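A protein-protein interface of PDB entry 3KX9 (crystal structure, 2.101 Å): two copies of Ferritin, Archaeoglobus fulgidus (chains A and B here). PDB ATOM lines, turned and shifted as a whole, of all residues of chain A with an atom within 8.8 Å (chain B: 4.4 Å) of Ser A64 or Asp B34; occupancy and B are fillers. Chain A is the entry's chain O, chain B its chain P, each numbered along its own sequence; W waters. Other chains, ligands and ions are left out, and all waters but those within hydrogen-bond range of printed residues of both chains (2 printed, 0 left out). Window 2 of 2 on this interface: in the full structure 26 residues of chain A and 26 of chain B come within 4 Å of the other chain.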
ATOM      1  N   ILE A   4       4.867 -34.305  -3.729  1.00  0.00           N
ATOM      2  CA  ILE A   4       4.766 -33.260  -2.718  1.00  0.00           C
ATOM      3  C   ILE A   4       4.063 -33.842  -1.494  1.00  0.00           C
ATOM      4  O   ILE A   4       3.001 -34.449  -1.625  1.00  0.00           O
ATOM      5  CB  ILE A   4       3.981 -32.036  -3.258  1.00  0.00           C
ATOM      6  CG1 ILE A   4       4.144 -30.833  -2.322  1.00  0.00           C
ATOM      7  CG2 ILE A   4       2.514 -32.382  -3.459  1.00  0.00           C
ATOM      8  CD1 ILE A   4       3.596 -29.543  -2.876  1.00  0.00           C
ATOM      9  N   VAL A   9       1.809 -29.456   1.378  1.00  0.00           N
ATOM     10  CA  VAL A   9       0.590 -28.902   0.814  1.00  0.00           C
ATOM     11  C   VAL A   9      -0.113 -28.067   1.882  1.00  0.00           C
ATOM     12  O   VAL A   9      -0.584 -26.967   1.607  1.00  0.00           O
ATOM     13  CB  VAL A   9      -0.342 -30.000   0.261  1.00  0.00           C
ATOM     14  CG1 VAL A   9      -1.739 -29.432  -0.014  1.00  0.00           C
ATOM     15  CG2 VAL A   9       0.256 -30.611  -1.003  1.00  0.00           C
ATOM     16  N   LEU A  12       1.810 -24.777   2.404  1.00  0.00           N
ATOM     17  CA  LEU A  12       1.581 -23.880   1.287  1.00  0.00           C
ATOM     18  C   LEU A  12       0.165 -23.297   1.326  1.00  0.00           C
ATOM     19  O   LEU A  12      -0.037 -22.120   1.043  1.00  0.00           O
ATOM     20  CB  LEU A  12       1.849 -24.601  -0.033  1.00  0.00           C
ATOM     21  CG  LEU A  12       3.342 -24.829  -0.280  1.00  0.00           C
ATOM     22  CD1 LEU A  12       3.560 -25.696  -1.496  1.00  0.00           C
ATOM     23  CD2 LEU A  12       4.039 -23.493  -0.436  1.00  0.00           C
ATOM     24  N   ASN A  13      -0.814 -24.118   1.685  1.00  0.00           N
ATOM     25  CA  ASN A  13      -2.179 -23.615   1.844  1.00  0.00           C
ATOM     26  C   ASN A  13      -2.250 -22.524   2.920  1.00  0.00           C
ATOM     27  O   ASN A  13      -2.972 -21.548   2.770  1.00  0.00           O
ATOM     28  CB  ASN A  13      -3.150 -24.772   2.138  1.00  0.00           C
ATOM     29  CG  ASN A  13      -3.391 -25.656   0.917  1.00  0.00           C
ATOM     30  OD1 ASN A  13      -3.109 -25.258  -0.214  1.00  0.00           O
ATOM     31  ND2 ASN A  13      -3.911 -26.860   1.143  1.00  0.00           N
ATOM     32  N   ILE A  16      -0.860 -19.489   1.418  1.00  0.00           N
ATOM     33  CA  ILE A  16      -1.855 -18.925   0.514  1.00  0.00           C
ATOM     34  C   ILE A  16      -2.784 -18.039   1.341  1.00  0.00           C
ATOM     35  O   ILE A  16      -3.122 -16.925   0.945  1.00  0.00           O
ATOM     36  CB  ILE A  16      -2.637 -20.018  -0.254  1.00  0.00           C
ATOM     37  CG1 ILE A  16      -1.703 -20.650  -1.302  1.00  0.00           C
ATOM     38  CG2 ILE A  16      -3.905 -19.420  -0.910  1.00  0.00           C
ATOM     39  CD1 ILE A  16      -2.323 -21.773  -2.140  1.00  0.00           C
ATOM     40  N   MET A  57      -2.509 -16.271  -5.908  1.00  0.00           N
ATOM     41  CA  MET A  57      -2.956 -17.082  -7.046  1.00  0.00           C
ATOM     42  C   MET A  57      -1.807 -17.877  -7.676  1.00  0.00           C
ATOM     43  O   MET A  57      -1.982 -19.029  -8.093  1.00  0.00           O
ATOM     44  CB  MET A  57      -3.619 -16.198  -8.104  1.00  0.00           C
ATOM     45  CG  MET A  57      -5.022 -15.691  -7.724  1.00  0.00           C
ATOM     46  SD  MET A  57      -6.113 -17.055  -7.261  1.00  0.00           S
ATOM     47  CE  MET A  57      -6.156 -16.820  -5.492  1.00  0.00           C
ATOM     48  N   LYS A  58      -0.632 -17.264  -7.746  1.00  0.00           N
ATOM     49  CA  LYS A  58       0.556 -17.974  -8.211  1.00  0.00           C
ATOM     50  C   LYS A  58       0.841 -19.222  -7.355  1.00  0.00           C
ATOM     51  O   LYS A  58       1.173 -20.294  -7.887  1.00  0.00           O
ATOM     52  CB  LYS A  58       1.756 -17.023  -8.218  1.00  0.00           C
ATOM     53  CG  LYS A  58       3.082 -17.646  -8.684  1.00  0.00           C
ATOM     54  CD  LYS A  58       4.259 -16.698  -8.347  1.00  0.00           C
ATOM     55  CE  LYS A  58       5.596 -17.196  -8.918  1.00  0.00           C
ATOM     56  NZ  LYS A  58       5.655 -17.113 -10.412  1.00  0.00           N
ATOM     57  N   MET A  59       0.692 -19.097  -6.036  1.00  0.00           N
ATOM     58  CA  MET A  59       0.916 -20.241  -5.141  1.00  0.00           C
ATOM     59  C   MET A  59      -0.237 -21.253  -5.229  1.00  0.00           C
ATOM     60  O   MET A  59      -0.020 -22.469  -5.194  1.00  0.00           O
ATOM     61  CB  MET A  59       1.139 -19.769  -3.690  1.00  0.00           C
ATOM     62  CG  MET A  59       1.583 -20.869  -2.711  1.00  0.00           C
ATOM     63  SD  MET A  59       2.191 -20.242  -1.112  1.00  0.00           S
ATOM     64  CE  MET A  59       3.800 -19.620  -1.589  1.00  0.00           C
ATOM     65  N   PHE A  60      -1.456 -20.734  -5.340  1.00  0.00           N
ATOM     66  CA  PHE A  60      -2.656 -21.532  -5.615  1.00  0.00           C
ATOM     67  C   PHE A  60      -2.443 -22.442  -6.843  1.00  0.00           C
ATOM     68  O   PHE A  60      -2.673 -23.653  -6.792  1.00  0.00           O
ATOM     69  CB  PHE A  60      -3.823 -20.573  -5.843  1.00  0.00           C
ATOM     70  CG  PHE A  60      -5.177 -21.235  -6.003  1.00  0.00           C
ATOM     71  CD1 PHE A  60      -6.075 -21.264  -4.946  1.00  0.00           C
ATOM     72  CD2 PHE A  60      -5.574 -21.757  -7.226  1.00  0.00           C
ATOM     73  CE1 PHE A  60      -7.329 -21.833  -5.096  1.00  0.00           C
ATOM     74  CE2 PHE A  60      -6.822 -22.324  -7.386  1.00  0.00           C
ATOM     75  CZ  PHE A  60      -7.710 -22.363  -6.325  1.00  0.00           C
ATOM     76  N   ASP A  61      -1.975 -21.863  -7.941  1.00  0.00           N
ATOM     77  CA  ASP A  61      -1.706 -22.652  -9.146  1.00  0.00           C
ATOM     78  C   ASP A  61      -0.597 -23.689  -8.948  1.00  0.00           C
ATOM     79  O   ASP A  61      -0.652 -24.784  -9.500  1.00  0.00           O
ATOM     80  CB  ASP A  61      -1.356 -21.740 -10.313  1.00  0.00           C
ATOM     81  CG  ASP A  61      -2.512 -20.832 -10.705  1.00  0.00           C
ATOM     82  OD1 ASP A  61      -3.678 -21.148 -10.367  1.00  0.00           O
ATOM     83  OD2 ASP A  61      -2.252 -19.800 -11.345  1.00  0.00           O
ATOM     84  N   PHE A  62       0.413 -23.344  -8.155  1.00  0.00           N
ATOM     85  CA  PHE A  62       1.525 -24.262  -7.917  1.00  0.00           C
ATOM     86  C   PHE A  62       1.096 -25.514  -7.147  1.00  0.00           C
ATOM     87  O   PHE A  62       1.461 -26.640  -7.511  1.00  0.00           O
ATOM     88  CB  PHE A  62       2.668 -23.550  -7.190  1.00  0.00           C
ATOM     89  CG  PHE A  62       3.865 -24.427  -6.914  1.00  0.00           C
ATOM     90  CD1 PHE A  62       4.771 -24.726  -7.923  1.00  0.00           C
ATOM     91  CD2 PHE A  62       4.096 -24.926  -5.637  1.00  0.00           C
ATOM     92  CE1 PHE A  62       5.891 -25.527  -7.662  1.00  0.00           C
ATOM     93  CE2 PHE A  62       5.208 -25.727  -5.366  1.00  0.00           C
ATOM     94  CZ  PHE A  62       6.104 -26.027  -6.373  1.00  0.00           C
ATOM     95  N   VAL A  63       0.347 -25.326  -6.071  1.00  0.00           N
ATOM     96  CA  VAL A  63      -0.090 -26.461  -5.261  1.00  0.00           C
ATOM     97  C   VAL A  63      -0.864 -27.434  -6.144  1.00  0.00           C
ATOM     98  O   VAL A  63      -0.666 -28.651  -6.094  1.00  0.00           O
ATOM     99  CB  VAL A  63      -0.991 -26.012  -4.084  1.00  0.00           C
ATOM    100  CG1 VAL A  63      -1.666 -27.224  -3.429  1.00  0.00           C
ATOM    101  CG2 VAL A  63      -0.178 -25.212  -3.056  1.00  0.00           C
ATOM    102  N   SER A  64      -1.744 -26.881  -6.963  1.00  0.00           N
ATOM    103  CA  SER A  64      -2.571 -27.688  -7.845  1.00  0.00           C
ATOM    104  C   SER A  64      -1.706 -28.383  -8.891  1.00  0.00           C
ATOM    105  O   SER A  64      -1.895 -29.560  -9.178  1.00  0.00           O
ATOM    106  CB  SER A  64      -3.640 -26.823  -8.515  1.00  0.00           C
ATOM    107  OG  SER A  64      -4.436 -27.619  -9.372  1.00  0.00           O
ATOM    108  N   GLU A  65      -0.736 -27.657  -9.440  1.00  0.00           N
ATOM    109  CA  GLU A  65       0.148 -28.218 -10.448  1.00  0.00           C
ATOM    110  C   GLU A  65       0.985 -29.379  -9.905  1.00  0.00           C
ATOM    111  O   GLU A  65       1.295 -30.308 -10.642  1.00  0.00           O
ATOM    112  CB  GLU A  65       1.056 -27.125 -11.021  1.00  0.00           C
ATOM    113  CG  GLU A  65       1.787 -27.502 -12.293  1.00  0.00           C
ATOM    114  CD  GLU A  65       2.731 -26.397 -12.767  1.00  0.00           C
ATOM    115  OE1 GLU A  65       3.203 -25.608 -11.919  1.00  0.00           O
ATOM    116  OE2 GLU A  65       3.002 -26.316 -13.986  1.00  0.00           O
ATOM    117  N   ARG A  66       1.346 -29.332  -8.624  1.00  0.00           N
ATOM    118  CA  ARG A  66       2.124 -30.412  -7.994  1.00  0.00           C
ATOM    119  C   ARG A  66       1.260 -31.613  -7.625  1.00  0.00           C
ATOM    120  O   ARG A  66       1.766 -32.612  -7.120  1.00  0.00           O
ATOM    121  CB  ARG A  66       2.845 -29.929  -6.732  1.00  0.00           C
ATOM    122  CG  ARG A  66       3.884 -28.842  -6.948  1.00  0.00           C
ATOM    123  CD  ARG A  66       5.102 -29.354  -7.695  1.00  0.00           C
ATOM    124  NE  ARG A  66       5.607 -30.609  -7.156  1.00  0.00           N
ATOM    125  CZ  ARG A  66       6.322 -30.733  -6.040  1.00  0.00           C
ATOM    126  NH1 ARG A  66       6.613 -29.671  -5.301  1.00  0.00           N
ATOM    127  NH2 ARG A  66       6.743 -31.936  -5.662  1.00  0.00           N
ATOM    128  N   GLY A  67      -0.041 -31.515  -7.870  1.00  0.00           N
ATOM    129  CA  GLY A  67      -0.950 -32.595  -7.524  1.00  0.00           C
ATOM    130  C   GLY A  67      -1.559 -32.445  -6.139  1.00  0.00           C
ATOM    131  O   GLY A  67      -2.216 -33.354  -5.626  1.00  0.00           O
ATOM    132  N   GLY A  68      -1.354 -31.289  -5.525  1.00  0.00           N
ATOM    133  CA  GLY A  68      -1.910 -31.049  -4.205  1.00  0.00           C
ATOM    134  C   GLY A  68      -3.280 -30.424  -4.325  1.00  0.00           C
ATOM    135  O   GLY A  68      -3.654 -29.924  -5.387  1.00  0.00           O
ATOM    136  N   ARG A  69      -4.027 -30.451  -3.228  1.00  0.00           N
ATOM    137  CA  ARG A  69      -5.375 -29.912  -3.207  1.00  0.00           C
ATOM    138  C   ARG A  69      -5.361 -28.627  -2.391  1.00  0.00           C
ATOM    139  O   ARG A  69      -4.988 -28.654  -1.220  1.00  0.00           O
ATOM    140  CB  ARG A  69      -6.320 -30.933  -2.569  1.00  0.00           C
ATOM    141  CG  ARG A  69      -7.737 -30.430  -2.355  1.00  0.00           C
ATOM    142  CD  ARG A  69      -8.386 -30.074  -3.662  1.00  0.00           C
ATOM    143  NE  ARG A  69      -9.787 -30.482  -3.702  1.00  0.00           N
ATOM    144  CZ  ARG A  69     -10.811 -29.653  -3.548  1.00  0.00           C
ATOM    145  NH1 ARG A  69     -10.603 -28.358  -3.348  1.00  0.00           N
ATOM    146  NH2 ARG A  69     -12.052 -30.116  -3.609  1.00  0.00           N
ATOM    147  N   VAL A  70      -5.732 -27.501  -3.003  1.00  0.00           N
ATOM    148  CA  VAL A  70      -5.776 -26.245  -2.254  1.00  0.00           C
ATOM    149  C   VAL A  70      -7.016 -26.201  -1.388  1.00  0.00           C
ATOM    150  O   VAL A  70      -8.136 -26.350  -1.875  1.00  0.00           O
ATOM    151  CB  VAL A  70      -5.746 -24.975  -3.143  1.00  0.00           C
ATOM    152  CG1 VAL A  70      -6.051 -23.747  -2.303  1.00  0.00           C
ATOM    153  CG2 VAL A  70      -4.389 -24.803  -3.813  1.00  0.00           C
ATOM    154  N   LYS A  71      -6.790 -25.978  -0.104  1.00  0.00           N
ATOM    155  CA  LYS A  71      -7.837 -25.884   0.898  1.00  0.00           C
ATOM    156  C   LYS A  71      -7.848 -24.444   1.395  1.00  0.00           C
ATOM    157  O   LYS A  71      -6.842 -23.977   1.923  1.00  0.00           O
ATOM    158  CB  LYS A  71      -7.453 -26.797   2.062  1.00  0.00           C
ATOM    159  CG  LYS A  71      -8.575 -27.571   2.673  1.00  0.00           C
ATOM    160  CD  LYS A  71      -9.576 -26.677   3.320  1.00  0.00           C
ATOM    161  CE  LYS A  71     -10.343 -27.441   4.385  1.00  0.00           C
ATOM    162  NZ  LYS A  71     -11.646 -26.799   4.681  1.00  0.00           N
ATOM    163  N   ALA B  30     -12.978 -23.460  -7.788  1.00  0.00           N
ATOM    164  CA  ALA B  30     -11.913 -23.541  -8.793  1.00  0.00           C
ATOM    165  C   ALA B  30     -10.878 -24.583  -8.387  1.00  0.00           C
ATOM    166  O   ALA B  30     -10.304 -25.278  -9.244  1.00  0.00           O
ATOM    167  CB  ALA B  30     -11.245 -22.195  -8.985  1.00  0.00           C
ATOM    168  N   SER B  31     -10.629 -24.667  -7.078  1.00  0.00           N
ATOM    169  CA  SER B  31      -9.747 -25.689  -6.518  1.00  0.00           C
ATOM    170  C   SER B  31     -10.361 -27.064  -6.717  1.00  0.00           C
ATOM    171  O   SER B  31      -9.683 -28.003  -7.138  1.00  0.00           O
ATOM    172  CB  SER B  31      -9.508 -25.456  -5.024  1.00  0.00           C
ATOM    173  OG  SER B  31      -8.866 -26.584  -4.445  1.00  0.00           O
ATOM    174  N   TYR B  32     -11.646 -27.175  -6.402  1.00  0.00           N
ATOM    175  CA  TYR B  32     -12.367 -28.433  -6.591  1.00  0.00           C
ATOM    176  C   TYR B  32     -12.379 -28.897  -8.049  1.00  0.00           C
ATOM    177  O   TYR B  32     -12.134 -30.069  -8.338  1.00  0.00           O
ATOM    178  CB  TYR B  32     -13.798 -28.346  -6.054  1.00  0.00           C
ATOM    179  CG  TYR B  32     -14.704 -29.443  -6.590  1.00  0.00           C
ATOM    180  CD1 TYR B  32     -14.558 -30.761  -6.175  1.00  0.00           C
ATOM    181  CD2 TYR B  32     -15.702 -29.159  -7.513  1.00  0.00           C
ATOM    182  CE1 TYR B  32     -15.382 -31.767  -6.671  1.00  0.00           C
ATOM    183  CE2 TYR B  32     -16.525 -30.147  -8.007  1.00  0.00           C
ATOM    184  CZ  TYR B  32     -16.365 -31.449  -7.584  1.00  0.00           C
ATOM    185  OH  TYR B  32     -17.192 -32.424  -8.085  1.00  0.00           O
ATOM    186  N   PHE B  33     -12.669 -27.983  -8.968  1.00  0.00           N
ATOM    187  CA  PHE B  33     -12.626 -28.337 -10.383  1.00  0.00           C
ATOM    188  C   PHE B  33     -11.227 -28.697 -10.838  1.00  0.00           C
ATOM    189  O   PHE B  33     -11.062 -29.650 -11.589  1.00  0.00           O
ATOM    190  CB  PHE B  33     -13.248 -27.250 -11.262  1.00  0.00           C
ATOM    191  CG  PHE B  33     -14.734 -27.270 -11.239  1.00  0.00           C
ATOM    192  CD1 PHE B  33     -15.447 -26.251 -10.632  1.00  0.00           C
ATOM    193  CD2 PHE B  33     -15.424 -28.344 -11.781  1.00  0.00           C
ATOM    194  CE1 PHE B  33     -16.822 -26.285 -10.582  1.00  0.00           C
ATOM    195  CE2 PHE B  33     -16.805 -28.383 -11.738  1.00  0.00           C
ATOM    196  CZ  PHE B  33     -17.504 -27.351 -11.133  1.00  0.00           C
ATOM    197  N   ASP B  34     -10.217 -27.950 -10.385  1.00  0.00           N
ATOM    198  CA  ASP B  34      -8.830 -28.328 -10.665  1.00  0.00           C
ATOM    199  C   ASP B  34      -8.547 -29.764 -10.204  1.00  0.00           C
ATOM    200  O   ASP B  34      -7.863 -30.524 -10.890  1.00  0.00           O
ATOM    201  CB  ASP B  34      -7.832 -27.383  -9.984  1.00  0.00           C
ATOM    202  CG  ASP B  34      -7.519 -26.145 -10.818  1.00  0.00           C
ATOM    203  OD1 ASP B  34      -7.773 -26.156 -12.044  1.00  0.00           O
ATOM    204  OD2 ASP B  34      -7.004 -25.158 -10.246  1.00  0.00           O
ATOM    205  N   SER B  35      -9.068 -30.122  -9.034  1.00  0.00           N
ATOM    206  CA  SER B  35      -8.780 -31.424  -8.456  1.00  0.00           C
ATOM    207  C   SER B  35      -9.358 -32.540  -9.309  1.00  0.00           C
ATOM    208  O   SER B  35      -8.746 -33.604  -9.435  1.00  0.00           O
ATOM    209  CB  SER B  35      -9.292 -31.525  -7.017  1.00  0.00           C
ATOM    210  OG  SER B  35     -10.679 -31.816  -6.976  1.00  0.00           O
ATOM    211  N   ILE B  36     -10.526 -32.318  -9.900  1.00  0.00           N
ATOM    212  CA  ILE B  36     -11.102 -33.355 -10.759  1.00  0.00           C
ATOM    213  C   ILE B  36     -10.776 -33.191 -12.254  1.00  0.00           C
ATOM    214  O   ILE B  36     -11.468 -33.746 -13.105  1.00  0.00           O
ATOM    215  CB  ILE B  36     -12.613 -33.512 -10.549  1.00  0.00           C
ATOM    216  CG1 ILE B  36     -13.353 -32.232 -10.937  1.00  0.00           C
ATOM    217  CG2 ILE B  36     -12.903 -33.866  -9.117  1.00  0.00           C
ATOM    218  CD1 ILE B  36     -14.856 -32.382 -10.944  1.00  0.00           C
ATOM    219  N   GLY B  37      -9.729 -32.432 -12.568  1.00  0.00           N
ATOM    220  CA  GLY B  37      -9.219 -32.355 -13.932  1.00  0.00           C
ATOM    221  C   GLY B  37     -10.060 -31.534 -14.902  1.00  0.00           C
ATOM    222  O   GLY B  37      -9.930 -31.661 -16.125  1.00  0.00           O
ATOM    223  N   LYS B  39     -10.236 -28.140 -15.947  1.00  0.00           N
ATOM    224  CA  LYS B  39      -9.590 -26.841 -15.930  1.00  0.00           C
ATOM    225  C   LYS B  39     -10.420 -25.739 -16.565  1.00  0.00           C
ATOM    226  O   LYS B  39     -10.232 -24.574 -16.240  1.00  0.00           O
ATOM    227  CB  LYS B  39      -8.202 -26.919 -16.557  1.00  0.00           C
ATOM    228  CG  LYS B  39      -7.263 -27.836 -15.765  1.00  0.00           C
ATOM    229  CD  LYS B  39      -5.887 -27.939 -16.392  1.00  0.00           C
ATOM    230  CE  LYS B  39      -5.068 -26.673 -16.156  1.00  0.00           C
ATOM    231  NZ  LYS B  39      -3.648 -26.828 -16.613  1.00  0.00           N
ATOM    232  N   SER B  42     -12.772 -24.768 -13.943  1.00  0.00           N
ATOM    233  CA  SER B  42     -11.949 -24.025 -12.998  1.00  0.00           C
ATOM    234  C   SER B  42     -11.803 -22.596 -13.494  1.00  0.00           C
ATOM    235  O   SER B  42     -11.967 -21.650 -12.724  1.00  0.00           O
ATOM    236  CB  SER B  42     -10.582 -24.683 -12.815  1.00  0.00           C
ATOM    237  OG  SER B  42      -9.851 -24.027 -11.803  1.00  0.00           O
ATOM    238  N   ARG B  46     -12.580 -18.974 -11.636  1.00  0.00           N
ATOM    239  CA  ARG B  46     -11.548 -17.961 -11.411  1.00  0.00           C
ATOM    240  C   ARG B  46     -11.968 -16.600 -11.958  1.00  0.00           C
ATOM    241  O   ARG B  46     -11.706 -15.570 -11.342  1.00  0.00           O
ATOM    242  CB  ARG B  46     -10.215 -18.401 -12.011  1.00  0.00           C
ATOM    243  CG  ARG B  46      -9.601 -19.621 -11.336  1.00  0.00           C
ATOM    244  CD  ARG B  46      -8.748 -20.386 -12.348  1.00  0.00           C
ATOM    245  NE  ARG B  46      -8.030 -21.533 -11.793  1.00  0.00           N
ATOM    246  CZ  ARG B  46      -6.843 -21.444 -11.202  1.00  0.00           C
ATOM    247  NH1 ARG B  46      -6.259 -20.256 -11.065  1.00  0.00           N
ATOM    248  NH2 ARG B  46      -6.245 -22.533 -10.743  1.00  0.00           N
HETATM  249  O   HOH W   1      -6.530 -27.437  -5.652  1.00  0.00           O
HETATM  250  O   HOH W   2      -5.801 -25.308  -7.435  1.00  0.00           O
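N of Ser B31 touches CZ of Phe A60 (3.8 Å). Arg B46 touches Phe A60. Ser A64 touches Asp B34. Arg A69 touches Ser B35 (NE to CB, 3.5 Å).
The backbone carbonyl oxygen of Arg A69 sits at hydrogen-bond distance from the side-chain amide nitrogen of Asn A13, at 3.2 Å. The backbone carbonyl oxygen of Tyr B32 lies within hydrogen-bond range of the side-chain hydroxyl of Ser B35, 2.7 Å away. The side-chain hydroxyl (OG) of Ser B42 lies within hydrogen-bond range of the side-chain carboxylate (OD1) of Asp B34. The side-chain carboxylate (OD2) of Asp B34 is in salt-bridge range of the guanidinium group (NH2) of Arg B46 (2.8 Å). OG of Ser B42 sits at hydrogen-bond distance from NE of Arg B46, 3.1 Å away.
Hydrophobic or aromatic side chains of chain A that line the printed part of chain B: Phe A60 and Val A70. Hydrophobic or aromatic side chains of chain B within 4 Å of the printed part of chain A: Tyr B32. Among the printed residues, Asp or Glu carboxylates within 4 Å of a Lys or Arg side-chain nitrogen of the other chain: Asp A61 with Arg B46 (2.8 Å).
Water W1 bridges OG of Ser B31 (2.8 Å) and N of Val A70 (2.8 Å). Water W2 lies within hydrogen-bond range of OD2 of Asp B34 and OG of Ser A64.
The side-chain carboxylate of Asp A61 is in salt-bridge range of the guanidinium group of Arg B46 (2.8 Å). The guanidinium group of Arg A69 lies within hydrogen-bond range of the side-chain hydroxyl of Ser B31. The side-chain hydroxyl (OG) of Ser B31 is in hydrogen-bond range of the backbone carbonyl oxygen (O) of Val A70, at 2.7 Å. The backbone NH (N) of Tyr B32 lies close to the guanidinium group (NH1) of Arg A69 (3.4 Å).
No position is printed for both chains. Of the 8 pairs that touch across the chains among the printed residues, none has its exchanged pair printed and touching as well.
Ser A64 touches one residue of chain B. Asp B34 touches one residue of chain A. Of the printed residues of chain A, Ser B35 touches Arg A69 (3.5 Å). Of the printed residues of chain B, Phe A60 touches Ser B31 (3.8 Å) and Arg B46 (3.4 Å). Of the printed residues of chain B, Val A70 touches Ser B31 (2.7 Å). Printed residues of chain B within 4 Å of Arg A69: Ser B31 (2.7 Å), Tyr B32 (3.4 Å) and Ser B35 (3.5 Å). Ile B36 touches none of the printed residues of chain A. Ala B30 touches none of the printed residues of chain A.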
